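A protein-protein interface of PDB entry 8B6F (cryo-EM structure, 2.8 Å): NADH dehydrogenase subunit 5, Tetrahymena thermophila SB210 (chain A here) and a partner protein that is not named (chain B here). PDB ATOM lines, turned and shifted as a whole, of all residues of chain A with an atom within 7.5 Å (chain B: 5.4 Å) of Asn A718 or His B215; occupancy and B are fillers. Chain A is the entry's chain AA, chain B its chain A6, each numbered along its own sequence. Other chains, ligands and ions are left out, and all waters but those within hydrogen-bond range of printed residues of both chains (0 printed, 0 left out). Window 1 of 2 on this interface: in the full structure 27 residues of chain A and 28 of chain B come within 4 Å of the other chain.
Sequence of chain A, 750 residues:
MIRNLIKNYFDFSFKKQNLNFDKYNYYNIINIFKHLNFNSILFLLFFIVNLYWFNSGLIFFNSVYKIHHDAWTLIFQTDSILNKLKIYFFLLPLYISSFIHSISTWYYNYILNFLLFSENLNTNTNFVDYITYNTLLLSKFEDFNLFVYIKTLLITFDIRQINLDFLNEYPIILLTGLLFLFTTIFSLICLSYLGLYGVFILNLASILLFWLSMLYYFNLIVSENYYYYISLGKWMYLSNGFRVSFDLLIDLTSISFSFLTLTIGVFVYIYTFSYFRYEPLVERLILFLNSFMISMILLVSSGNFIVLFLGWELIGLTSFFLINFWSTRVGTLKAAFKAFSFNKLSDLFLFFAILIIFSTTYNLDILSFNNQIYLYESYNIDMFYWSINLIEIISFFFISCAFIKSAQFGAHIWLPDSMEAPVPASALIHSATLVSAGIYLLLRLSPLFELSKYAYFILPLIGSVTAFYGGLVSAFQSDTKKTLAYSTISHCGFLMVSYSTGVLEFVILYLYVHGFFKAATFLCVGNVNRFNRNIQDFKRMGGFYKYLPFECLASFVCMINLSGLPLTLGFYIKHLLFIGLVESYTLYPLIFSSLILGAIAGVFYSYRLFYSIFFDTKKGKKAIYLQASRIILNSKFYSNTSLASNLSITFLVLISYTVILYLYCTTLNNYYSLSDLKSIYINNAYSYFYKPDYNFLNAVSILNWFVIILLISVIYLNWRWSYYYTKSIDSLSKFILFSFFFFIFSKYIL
NE2 of His B215 sits at hydrogen-bond distance from O of Asn A718, at 3.3 Å. The side-chain hydroxyl (OH) of Tyr A725 sits at hydrogen-bond distance from the backbone carbonyl oxygen (O) of Gly B213 (2.9 Å). The backbone carbonyl oxygen (O) of Asn A718 lies close to the backbone carbonyl oxygen (O) of Ile B212, at 3.5 Å.
The backbone carbonyl oxygen (O) of Tyr A716 lies close to the side-chain amide oxygen (OD1) of Asn A718. OG of Ser A722 is in hydrogen-bond range of O of Arg A720 (3.5 Å). The backbone carbonyl oxygen (O) of Ala B211 is in hydrogen-bond range of a ring nitrogen (NE2) of His B215, 2.9 Å away. O of His B215 sits at hydrogen-bond distance from NH1 of Arg B236 (2.6 Å). The backbone carbonyl oxygen (O) of Gly B216 sits at hydrogen-bond distance from the backbone NH (N) of Arg B236 (3.1 Å).
Among the printed residues, pairs that only touch across the chains: Trp A719 with His B215, Tyr A725 with Gly B216, Trp A721 with His B215, Trp A719 with Ile B212, Asn A718 with Ala B211, Leu A717 with Ile B212, Arg A720 with His B215, Tyr A716 with Lys B152, Trp A721 with Arg B236, Trp A719 with Ala B211, Leu A717 with Lys B152, Tyr A725 with Lys B152 and Tyr A725 with His B215.
Of chain B, only Ala B211, Ile B212 and His B215 come within 4 Å of Asn A718. Printed residues of chain B within 4 Å of Trp A719: Ala B211 (3.8 Å), Ile B212 (3.6 Å) and His B215 (3.4 Å). Printed residues of chain B within 4 Å of Trp A721: His B215 and Arg B236. Of the printed residues of chain B, Tyr A725 touches Lys B152 (3.96 Å), Gly B213 (2.9 Å), His B215 (3.97 Å) and Gly B216 (3.4 Å). Printed residues of chain A within 4 Å of Gly B213: Tyr A725 (2.9 Å). No residue of chain A comes within 4 Å of Gly B214. Of the printed residues of chain A, Gly B216 touches Tyr A725. The nearest residue of chain A that does not touch His B215 is Ser A722 (5.4 Å).
Hydrophobic or aromatic side chains of chain B that line the printed part of chain A: Ile B212 and His B215. Along chain A the printed residues that touch a printed residue of chain B span positions 716 to 725. Among the printed residues, 16 pairs touch across the chains. Among the printed residues, no Asp or Glu carboxylate lies within 4 Å of a Lys or Arg side-chain nitrogen of the other chain.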
ATOM      1  N   SER A 713       9.282 -26.172 -19.782  1.00  0.00           N
ATOM      2  CA  SER A 713       8.514 -26.433 -20.995  1.00  0.00           C
ATOM      3  C   SER A 713       7.019 -26.478 -20.706  1.00  0.00           C
ATOM      4  O   SER A 713       6.227 -25.803 -21.372  1.00  0.00           O
ATOM      5  CB  SER A 713       8.968 -27.749 -21.626  1.00  0.00           C
ATOM      6  OG  SER A 713       8.449 -28.860 -20.915  1.00  0.00           O
ATOM      7  N   VAL A 714       6.610 -27.264 -19.710  1.00  0.00           N
ATOM      8  CA  VAL A 714       5.186 -27.393 -19.429  1.00  0.00           C
ATOM      9  C   VAL A 714       4.584 -26.088 -18.929  1.00  0.00           C
ATOM     10  O   VAL A 714       3.366 -25.899 -19.025  1.00  0.00           O
ATOM     11  CB  VAL A 714       4.927 -28.522 -18.411  1.00  0.00           C
ATOM     12  CG1 VAL A 714       5.389 -29.860 -18.969  1.00  0.00           C
ATOM     13  CG2 VAL A 714       5.614 -28.228 -17.090  1.00  0.00           C
ATOM     14  N   ILE A 715       5.394 -25.177 -18.396  1.00  0.00           N
ATOM     15  CA  ILE A 715       4.871 -23.914 -17.885  1.00  0.00           C
ATOM     16  C   ILE A 715       4.822 -22.844 -18.969  1.00  0.00           C
ATOM     17  O   ILE A 715       3.772 -22.249 -19.218  1.00  0.00           O
ATOM     18  CB  ILE A 715       5.715 -23.455 -16.675  1.00  0.00           C
ATOM     19  CG1 ILE A 715       5.426 -24.355 -15.471  1.00  0.00           C
ATOM     20  CG2 ILE A 715       5.427 -21.992 -16.335  1.00  0.00           C
ATOM     21  CD1 ILE A 715       6.302 -24.089 -14.272  1.00  0.00           C
ATOM     22  N   TYR A 716       5.945 -22.578 -19.630  1.00  0.00           N
ATOM     23  CA  TYR A 716       6.053 -21.431 -20.524  1.00  0.00           C
ATOM     24  C   TYR A 716       5.744 -21.751 -21.980  1.00  0.00           C
ATOM     25  O   TYR A 716       5.812 -20.846 -22.817  1.00  0.00           O
ATOM     26  CB  TYR A 716       7.457 -20.827 -20.441  1.00  0.00           C
ATOM     27  CG  TYR A 716       7.642 -19.842 -19.314  1.00  0.00           C
ATOM     28  CD1 TYR A 716       7.083 -18.574 -19.384  1.00  0.00           C
ATOM     29  CD2 TYR A 716       8.394 -20.167 -18.194  1.00  0.00           C
ATOM     30  CE1 TYR A 716       7.253 -17.664 -18.367  1.00  0.00           C
ATOM     31  CE2 TYR A 716       8.572 -19.259 -17.168  1.00  0.00           C
ATOM     32  CZ  TYR A 716       8.001 -18.008 -17.264  1.00  0.00           C
ATOM     33  OH  TYR A 716       8.166 -17.088 -16.253  1.00  0.00           O
ATOM     34  N   LEU A 717       5.405 -22.991 -22.310  1.00  0.00           N
ATOM     35  CA  LEU A 717       5.171 -23.371 -23.697  1.00  0.00           C
ATOM     36  C   LEU A 717       3.727 -23.082 -24.081  1.00  0.00           C
ATOM     37  O   LEU A 717       2.798 -23.480 -23.373  1.00  0.00           O
ATOM     38  CB  LEU A 717       5.500 -24.848 -23.912  1.00  0.00           C
ATOM     39  CG  LEU A 717       5.505 -25.351 -25.355  1.00  0.00           C
ATOM     40  CD1 LEU A 717       6.533 -24.602 -26.182  1.00  0.00           C
ATOM     41  CD2 LEU A 717       5.782 -26.843 -25.397  1.00  0.00           C
ATOM     42  N   ASN A 718       3.543 -22.386 -25.200  1.00  0.00           N
ATOM     43  CA  ASN A 718       2.224 -22.000 -25.680  1.00  0.00           C
ATOM     44  C   ASN A 718       1.810 -22.904 -26.832  1.00  0.00           C
ATOM     45  O   ASN A 718       2.549 -23.053 -27.809  1.00  0.00           O
ATOM     46  CB  ASN A 718       2.211 -20.540 -26.136  1.00  0.00           C
ATOM     47  CG  ASN A 718       2.376 -19.570 -24.988  1.00  0.00           C
ATOM     48  OD1 ASN A 718       3.493 -19.249 -24.585  1.00  0.00           O
ATOM     49  ND2 ASN A 718       1.257 -19.089 -24.457  1.00  0.00           N
ATOM     50  N   TRP A 719       0.624 -23.501 -26.712  1.00  0.00           N
ATOM     51  CA  TRP A 719       0.058 -24.330 -27.765  1.00  0.00           C
ATOM     52  C   TRP A 719      -1.130 -23.681 -28.458  1.00  0.00           C
ATOM     53  O   TRP A 719      -1.553 -24.170 -29.511  1.00  0.00           O
ATOM     54  CB  TRP A 719      -0.372 -25.690 -27.197  1.00  0.00           C
ATOM     55  CG  TRP A 719       0.765 -26.516 -26.688  1.00  0.00           C
ATOM     56  CD1 TRP A 719       1.211 -26.593 -25.402  1.00  0.00           C
ATOM     57  CD2 TRP A 719       1.602 -27.385 -27.457  1.00  0.00           C
ATOM     58  NE1 TRP A 719       2.276 -27.456 -25.323  1.00  0.00           N
ATOM     59  CE2 TRP A 719       2.536 -27.957 -26.572  1.00  0.00           C
ATOM     60  CE3 TRP A 719       1.655 -27.735 -28.809  1.00  0.00           C
ATOM     61  CZ2 TRP A 719       3.509 -28.858 -26.993  1.00  0.00           C
ATOM     62  CZ3 TRP A 719       2.620 -28.629 -29.228  1.00  0.00           C
ATOM     63  CH2 TRP A 719       3.536 -29.182 -28.322  1.00  0.00           C
ATOM     64  N   ARG A 720      -1.677 -22.607 -27.900  1.00  0.00           N
ATOM     65  CA  ARG A 720      -2.834 -21.925 -28.458  1.00  0.00           C
ATOM     66  C   ARG A 720      -2.593 -20.425 -28.438  1.00  0.00           C
ATOM     67  O   ARG A 720      -1.893 -19.905 -27.564  1.00  0.00           O
ATOM     68  CB  ARG A 720      -4.105 -22.252 -27.672  1.00  0.00           C
ATOM     69  CG  ARG A 720      -4.027 -21.860 -26.207  1.00  0.00           C
ATOM     70  CD  ARG A 720      -5.201 -22.413 -25.426  1.00  0.00           C
ATOM     71  NE  ARG A 720      -5.043 -22.204 -23.993  1.00  0.00           N
ATOM     72  CZ  ARG A 720      -5.844 -22.715 -23.069  1.00  0.00           C
ATOM     73  NH1 ARG A 720      -6.873 -23.480 -23.392  1.00  0.00           N
ATOM     74  NH2 ARG A 720      -5.603 -22.456 -21.787  1.00  0.00           N
ATOM     75  N   TRP A 721      -3.178 -19.729 -29.407  1.00  0.00           N
ATOM     76  CA  TRP A 721      -3.076 -18.278 -29.436  1.00  0.00           C
ATOM     77  C   TRP A 721      -3.746 -17.686 -28.204  1.00  0.00           C
ATOM     78  O   TRP A 721      -4.783 -18.171 -27.746  1.00  0.00           O
ATOM     79  CB  TRP A 721      -3.716 -17.717 -30.705  1.00  0.00           C
ATOM     80  CG  TRP A 721      -3.719 -16.221 -30.742  1.00  0.00           C
ATOM     81  CD1 TRP A 721      -2.761 -15.415 -31.279  1.00  0.00           C
ATOM     82  CD2 TRP A 721      -4.725 -15.350 -30.209  1.00  0.00           C
ATOM     83  NE1 TRP A 721      -3.108 -14.097 -31.118  1.00  0.00           N
ATOM     84  CE2 TRP A 721      -4.309 -14.030 -30.464  1.00  0.00           C
ATOM     85  CE3 TRP A 721      -5.936 -15.560 -29.543  1.00  0.00           C
ATOM     86  CZ2 TRP A 721      -5.062 -12.923 -30.079  1.00  0.00           C
ATOM     87  CZ3 TRP A 721      -6.683 -14.460 -29.160  1.00  0.00           C
ATOM     88  CH2 TRP A 721      -6.242 -13.157 -29.428  1.00  0.00           C
ATOM     89  N   SER A 722      -3.143 -16.630 -27.667  1.00  0.00           N
ATOM     90  CA  SER A 722      -3.669 -15.971 -26.482  1.00  0.00           C
ATOM     91  C   SER A 722      -3.304 -14.498 -26.530  1.00  0.00           C
ATOM     92  O   SER A 722      -2.373 -14.088 -27.227  1.00  0.00           O
ATOM     93  CB  SER A 722      -3.124 -16.602 -25.196  1.00  0.00           C
ATOM     94  OG  SER A 722      -3.440 -17.980 -25.129  1.00  0.00           O
ATOM     95  N   TYR A 724      -1.887 -13.112 -24.242  1.00  0.00           N
ATOM     96  CA  TYR A 724      -0.712 -13.004 -23.387  1.00  0.00           C
ATOM     97  C   TYR A 724       0.503 -13.701 -23.989  1.00  0.00           C
ATOM     98  O   TYR A 724       1.430 -14.064 -23.261  1.00  0.00           O
ATOM     99  CB  TYR A 724      -1.033 -13.586 -22.007  1.00  0.00           C
ATOM    100  CG  TYR A 724      -0.094 -13.160 -20.901  1.00  0.00           C
ATOM    101  CD1 TYR A 724      -0.208 -11.911 -20.306  1.00  0.00           C
ATOM    102  CD2 TYR A 724       0.887 -14.023 -20.430  1.00  0.00           C
ATOM    103  CE1 TYR A 724       0.643 -11.524 -19.289  1.00  0.00           C
ATOM    104  CE2 TYR A 724       1.743 -13.646 -19.414  1.00  0.00           C
ATOM    105  CZ  TYR A 724       1.617 -12.396 -18.848  1.00  0.00           C
ATOM    106  OH  TYR A 724       2.467 -12.022 -17.834  1.00  0.00           O
ATOM    107  N   TYR A 725       0.524 -13.888 -25.310  1.00  0.00           N
ATOM    108  CA  TYR A 725       1.652 -14.569 -25.937  1.00  0.00           C
ATOM    109  C   TYR A 725       2.934 -13.756 -25.799  1.00  0.00           C
ATOM    110  O   TYR A 725       3.957 -14.266 -25.329  1.00  0.00           O
ATOM    111  CB  TYR A 725       1.340 -14.840 -27.409  1.00  0.00           C
ATOM    112  CG  TYR A 725       2.457 -15.532 -28.156  1.00  0.00           C
ATOM    113  CD1 TYR A 725       2.711 -16.884 -27.972  1.00  0.00           C
ATOM    114  CD2 TYR A 725       3.244 -14.835 -29.063  1.00  0.00           C
ATOM    115  CE1 TYR A 725       3.729 -17.518 -28.658  1.00  0.00           C
ATOM    116  CE2 TYR A 725       4.263 -15.461 -29.753  1.00  0.00           C
ATOM    117  CZ  TYR A 725       4.499 -16.802 -29.547  1.00  0.00           C
ATOM    118  OH  TYR A 725       5.513 -17.428 -30.234  1.00  0.00           O
ATOM    119  N   THR A 726       2.897 -12.485 -26.201  1.00  0.00           N
ATOM    120  CA  THR A 726       4.096 -11.656 -26.132  1.00  0.00           C
ATOM    121  C   THR A 726       4.533 -11.438 -24.690  1.00  0.00           C
ATOM    122  O   THR A 726       5.726 -11.517 -24.376  1.00  0.00           O
ATOM    123  CB  THR A 726       3.849 -10.313 -26.821  1.00  0.00           C
ATOM    124  OG1 THR A 726       2.888  -9.556 -26.073  1.00  0.00           O
ATOM    125  CG2 THR A 726       3.334 -10.521 -28.238  1.00  0.00           C
ATOM    126  N   SER A 728       3.964 -13.412 -22.232  1.00  0.00           N
ATOM    127  CA  SER A 728       4.499 -14.673 -21.733  1.00  0.00           C
ATOM    128  C   SER A 728       5.957 -14.852 -22.135  1.00  0.00           C
ATOM    129  O   SER A 728       6.783 -15.271 -21.317  1.00  0.00           O
ATOM    130  CB  SER A 728       3.654 -15.836 -22.251  1.00  0.00           C
ATOM    131  OG  SER A 728       4.246 -17.079 -21.921  1.00  0.00           O
ATOM    132  N   ILE A 729       6.294 -14.553 -23.391  1.00  0.00           N
ATOM    133  CA  ILE A 729       7.691 -14.615 -23.814  1.00  0.00           C
ATOM    134  C   ILE A 729       8.526 -13.634 -23.004  1.00  0.00           C
ATOM    135  O   ILE A 729       9.646 -13.945 -22.584  1.00  0.00           O
ATOM    136  CB  ILE A 729       7.809 -14.349 -25.326  1.00  0.00           C
ATOM    137  CG1 ILE A 729       7.128 -15.475 -26.107  1.00  0.00           C
ATOM    138  CG2 ILE A 729       9.276 -14.210 -25.733  1.00  0.00           C
ATOM    139  CD1 ILE A 729       7.134 -15.285 -27.609  1.00  0.00           C
ATOM    140  N   LYS B 152      10.331 -22.733 -31.131  1.00  0.00           N
ATOM    141  CA  LYS B 152       9.490 -21.917 -30.263  1.00  0.00           C
ATOM    142  C   LYS B 152       9.688 -20.430 -30.526  1.00  0.00           C
ATOM    143  O   LYS B 152       8.719 -19.694 -30.742  1.00  0.00           O
ATOM    144  CB  LYS B 152       9.788 -22.254 -28.801  1.00  0.00           C
ATOM    145  CG  LYS B 152       9.032 -21.410 -27.788  1.00  0.00           C
ATOM    146  CD  LYS B 152       9.338 -21.868 -26.371  1.00  0.00           C
ATOM    147  CE  LYS B 152       8.636 -21.007 -25.338  1.00  0.00           C
ATOM    148  NZ  LYS B 152       9.108 -19.597 -25.368  1.00  0.00           N
ATOM    149  N   TRP B 210       4.731 -23.721 -36.282  1.00  0.00           N
ATOM    150  CA  TRP B 210       3.425 -23.104 -36.098  1.00  0.00           C
ATOM    151  C   TRP B 210       2.709 -23.635 -34.866  1.00  0.00           C
ATOM    152  O   TRP B 210       1.821 -22.956 -34.340  1.00  0.00           O
ATOM    153  CB  TRP B 210       2.565 -23.328 -37.343  1.00  0.00           C
ATOM    154  CG  TRP B 210       3.201 -22.793 -38.584  1.00  0.00           C
ATOM    155  CD1 TRP B 210       3.722 -23.519 -39.615  1.00  0.00           C
ATOM    156  CD2 TRP B 210       3.405 -21.417 -38.918  1.00  0.00           C
ATOM    157  NE1 TRP B 210       4.231 -22.678 -40.573  1.00  0.00           N
ATOM    158  CE2 TRP B 210       4.048 -21.381 -40.170  1.00  0.00           C
ATOM    159  CE3 TRP B 210       3.100 -20.209 -38.281  1.00  0.00           C
ATOM    160  CZ2 TRP B 210       4.392 -20.188 -40.798  1.00  0.00           C
ATOM    161  CZ3 TRP B 210       3.442 -19.025 -38.905  1.00  0.00           C
ATOM    162  CH2 TRP B 210       4.083 -19.022 -40.152  1.00  0.00           C
ATOM    163  N   ALA B 211       3.075 -24.827 -34.392  1.00  0.00           N
ATOM    164  CA  ALA B 211       2.412 -25.393 -33.222  1.00  0.00           C
ATOM    165  C   ALA B 211       2.763 -24.626 -31.952  1.00  0.00           C
ATOM    166  O   ALA B 211       1.878 -24.330 -31.142  1.00  0.00           O
ATOM    167  CB  ALA B 211       2.783 -26.868 -33.071  1.00  0.00           C
ATOM    168  N   ILE B 212       4.038 -24.297 -31.755  1.00  0.00           N
ATOM    169  CA  ILE B 212       4.501 -23.742 -30.486  1.00  0.00           C
ATOM    170  C   ILE B 212       5.021 -22.318 -30.596  1.00  0.00           C
ATOM    171  O   ILE B 212       5.193 -21.665 -29.555  1.00  0.00           O
ATOM    172  CB  ILE B 212       5.581 -24.636 -29.837  1.00  0.00           C
ATOM    173  CG1 ILE B 212       6.793 -24.785 -30.759  1.00  0.00           C
ATOM    174  CG2 ILE B 212       5.002 -25.997 -29.495  1.00  0.00           C
ATOM    175  CD1 ILE B 212       7.986 -25.428 -30.091  1.00  0.00           C
ATOM    176  N   GLY B 213       5.290 -21.803 -31.794  1.00  0.00           N
ATOM    177  CA  GLY B 213       5.909 -20.494 -31.899  1.00  0.00           C
ATOM    178  C   GLY B 213       5.284 -19.545 -32.901  1.00  0.00           C
ATOM    179  O   GLY B 213       5.630 -18.361 -32.929  1.00  0.00           O
ATOM    180  N   GLY B 214       4.369 -20.036 -33.724  1.00  0.00           N
ATOM    181  CA  GLY B 214       3.769 -19.238 -34.771  1.00  0.00           C
ATOM    182  C   GLY B 214       2.553 -18.440 -34.359  1.00  0.00           C
ATOM    183  O   GLY B 214       1.906 -17.837 -35.221  1.00  0.00           O
ATOM    184  N   HIS B 215       2.216 -18.413 -33.069  1.00  0.00           N
ATOM    185  CA  HIS B 215       0.988 -17.748 -32.642  1.00  0.00           C
ATOM    186  C   HIS B 215       1.096 -16.235 -32.768  1.00  0.00           C
ATOM    187  O   HIS B 215       0.113 -15.564 -33.103  1.00  0.00           O
ATOM    188  CB  HIS B 215       0.662 -18.144 -31.204  1.00  0.00           C
ATOM    189  CG  HIS B 215       0.673 -19.622 -30.971  1.00  0.00           C
ATOM    190  ND1 HIS B 215      -0.222 -20.478 -31.576  1.00  0.00           N
ATOM    191  CD2 HIS B 215       1.475 -20.396 -30.205  1.00  0.00           C
ATOM    192  CE1 HIS B 215       0.029 -21.717 -31.191  1.00  0.00           C
ATOM    193  NE2 HIS B 215       1.053 -21.694 -30.359  1.00  0.00           N
ATOM    194  N   GLY B 216       2.275 -15.676 -32.499  1.00  0.00           N
ATOM    195  CA  GLY B 216       2.417 -14.229 -32.529  1.00  0.00           C
ATOM    196  C   GLY B 216       2.207 -13.641 -33.911  1.00  0.00           C
ATOM    197  O   GLY B 216       1.604 -12.577 -34.057  1.00  0.00           O
ATOM    198  N   VAL B 217       2.699 -14.323 -34.941  1.00  0.00           N
ATOM    199  CA  VAL B 217       2.671 -13.803 -36.299  1.00  0.00           C
ATOM    200  C   VAL B 217       1.430 -14.318 -37.019  1.00  0.00           C
ATOM    201  O   VAL B 217       0.830 -15.325 -36.638  1.00  0.00           O
ATOM    202  CB  VAL B 217       3.955 -14.179 -37.064  1.00  0.00           C
ATOM    203  CG1 VAL B 217       5.180 -13.699 -36.301  1.00  0.00           C
ATOM    204  CG2 VAL B 217       4.026 -15.682 -37.302  1.00  0.00           C
ATOM    205  N   ARG B 236       0.683  -9.998 -35.596  1.00  0.00           N
ATOM    206  CA  ARG B 236      -0.759  -9.776 -35.567  1.00  0.00           C
ATOM    207  C   ARG B 236      -1.092  -8.412 -34.980  1.00  0.00           C
ATOM    208  O   ARG B 236      -1.954  -7.696 -35.501  1.00  0.00           O
ATOM    209  CB  ARG B 236      -1.446 -10.882 -34.768  1.00  0.00           C
ATOM    210  CG  ARG B 236      -1.662 -12.167 -35.546  1.00  0.00           C
ATOM    211  CD  ARG B 236      -2.487 -13.157 -34.744  1.00  0.00           C
ATOM    212  NE  ARG B 236      -3.019 -14.225 -35.581  1.00  0.00           N
ATOM    213  CZ  ARG B 236      -2.378 -15.349 -35.868  1.00  0.00           C
ATOM    214  NH1 ARG B 236      -1.164 -15.593 -35.404  1.00  0.00           N
ATOM    215  NH2 ARG B 236      -2.970 -16.253 -36.643  1.00  0.00           N
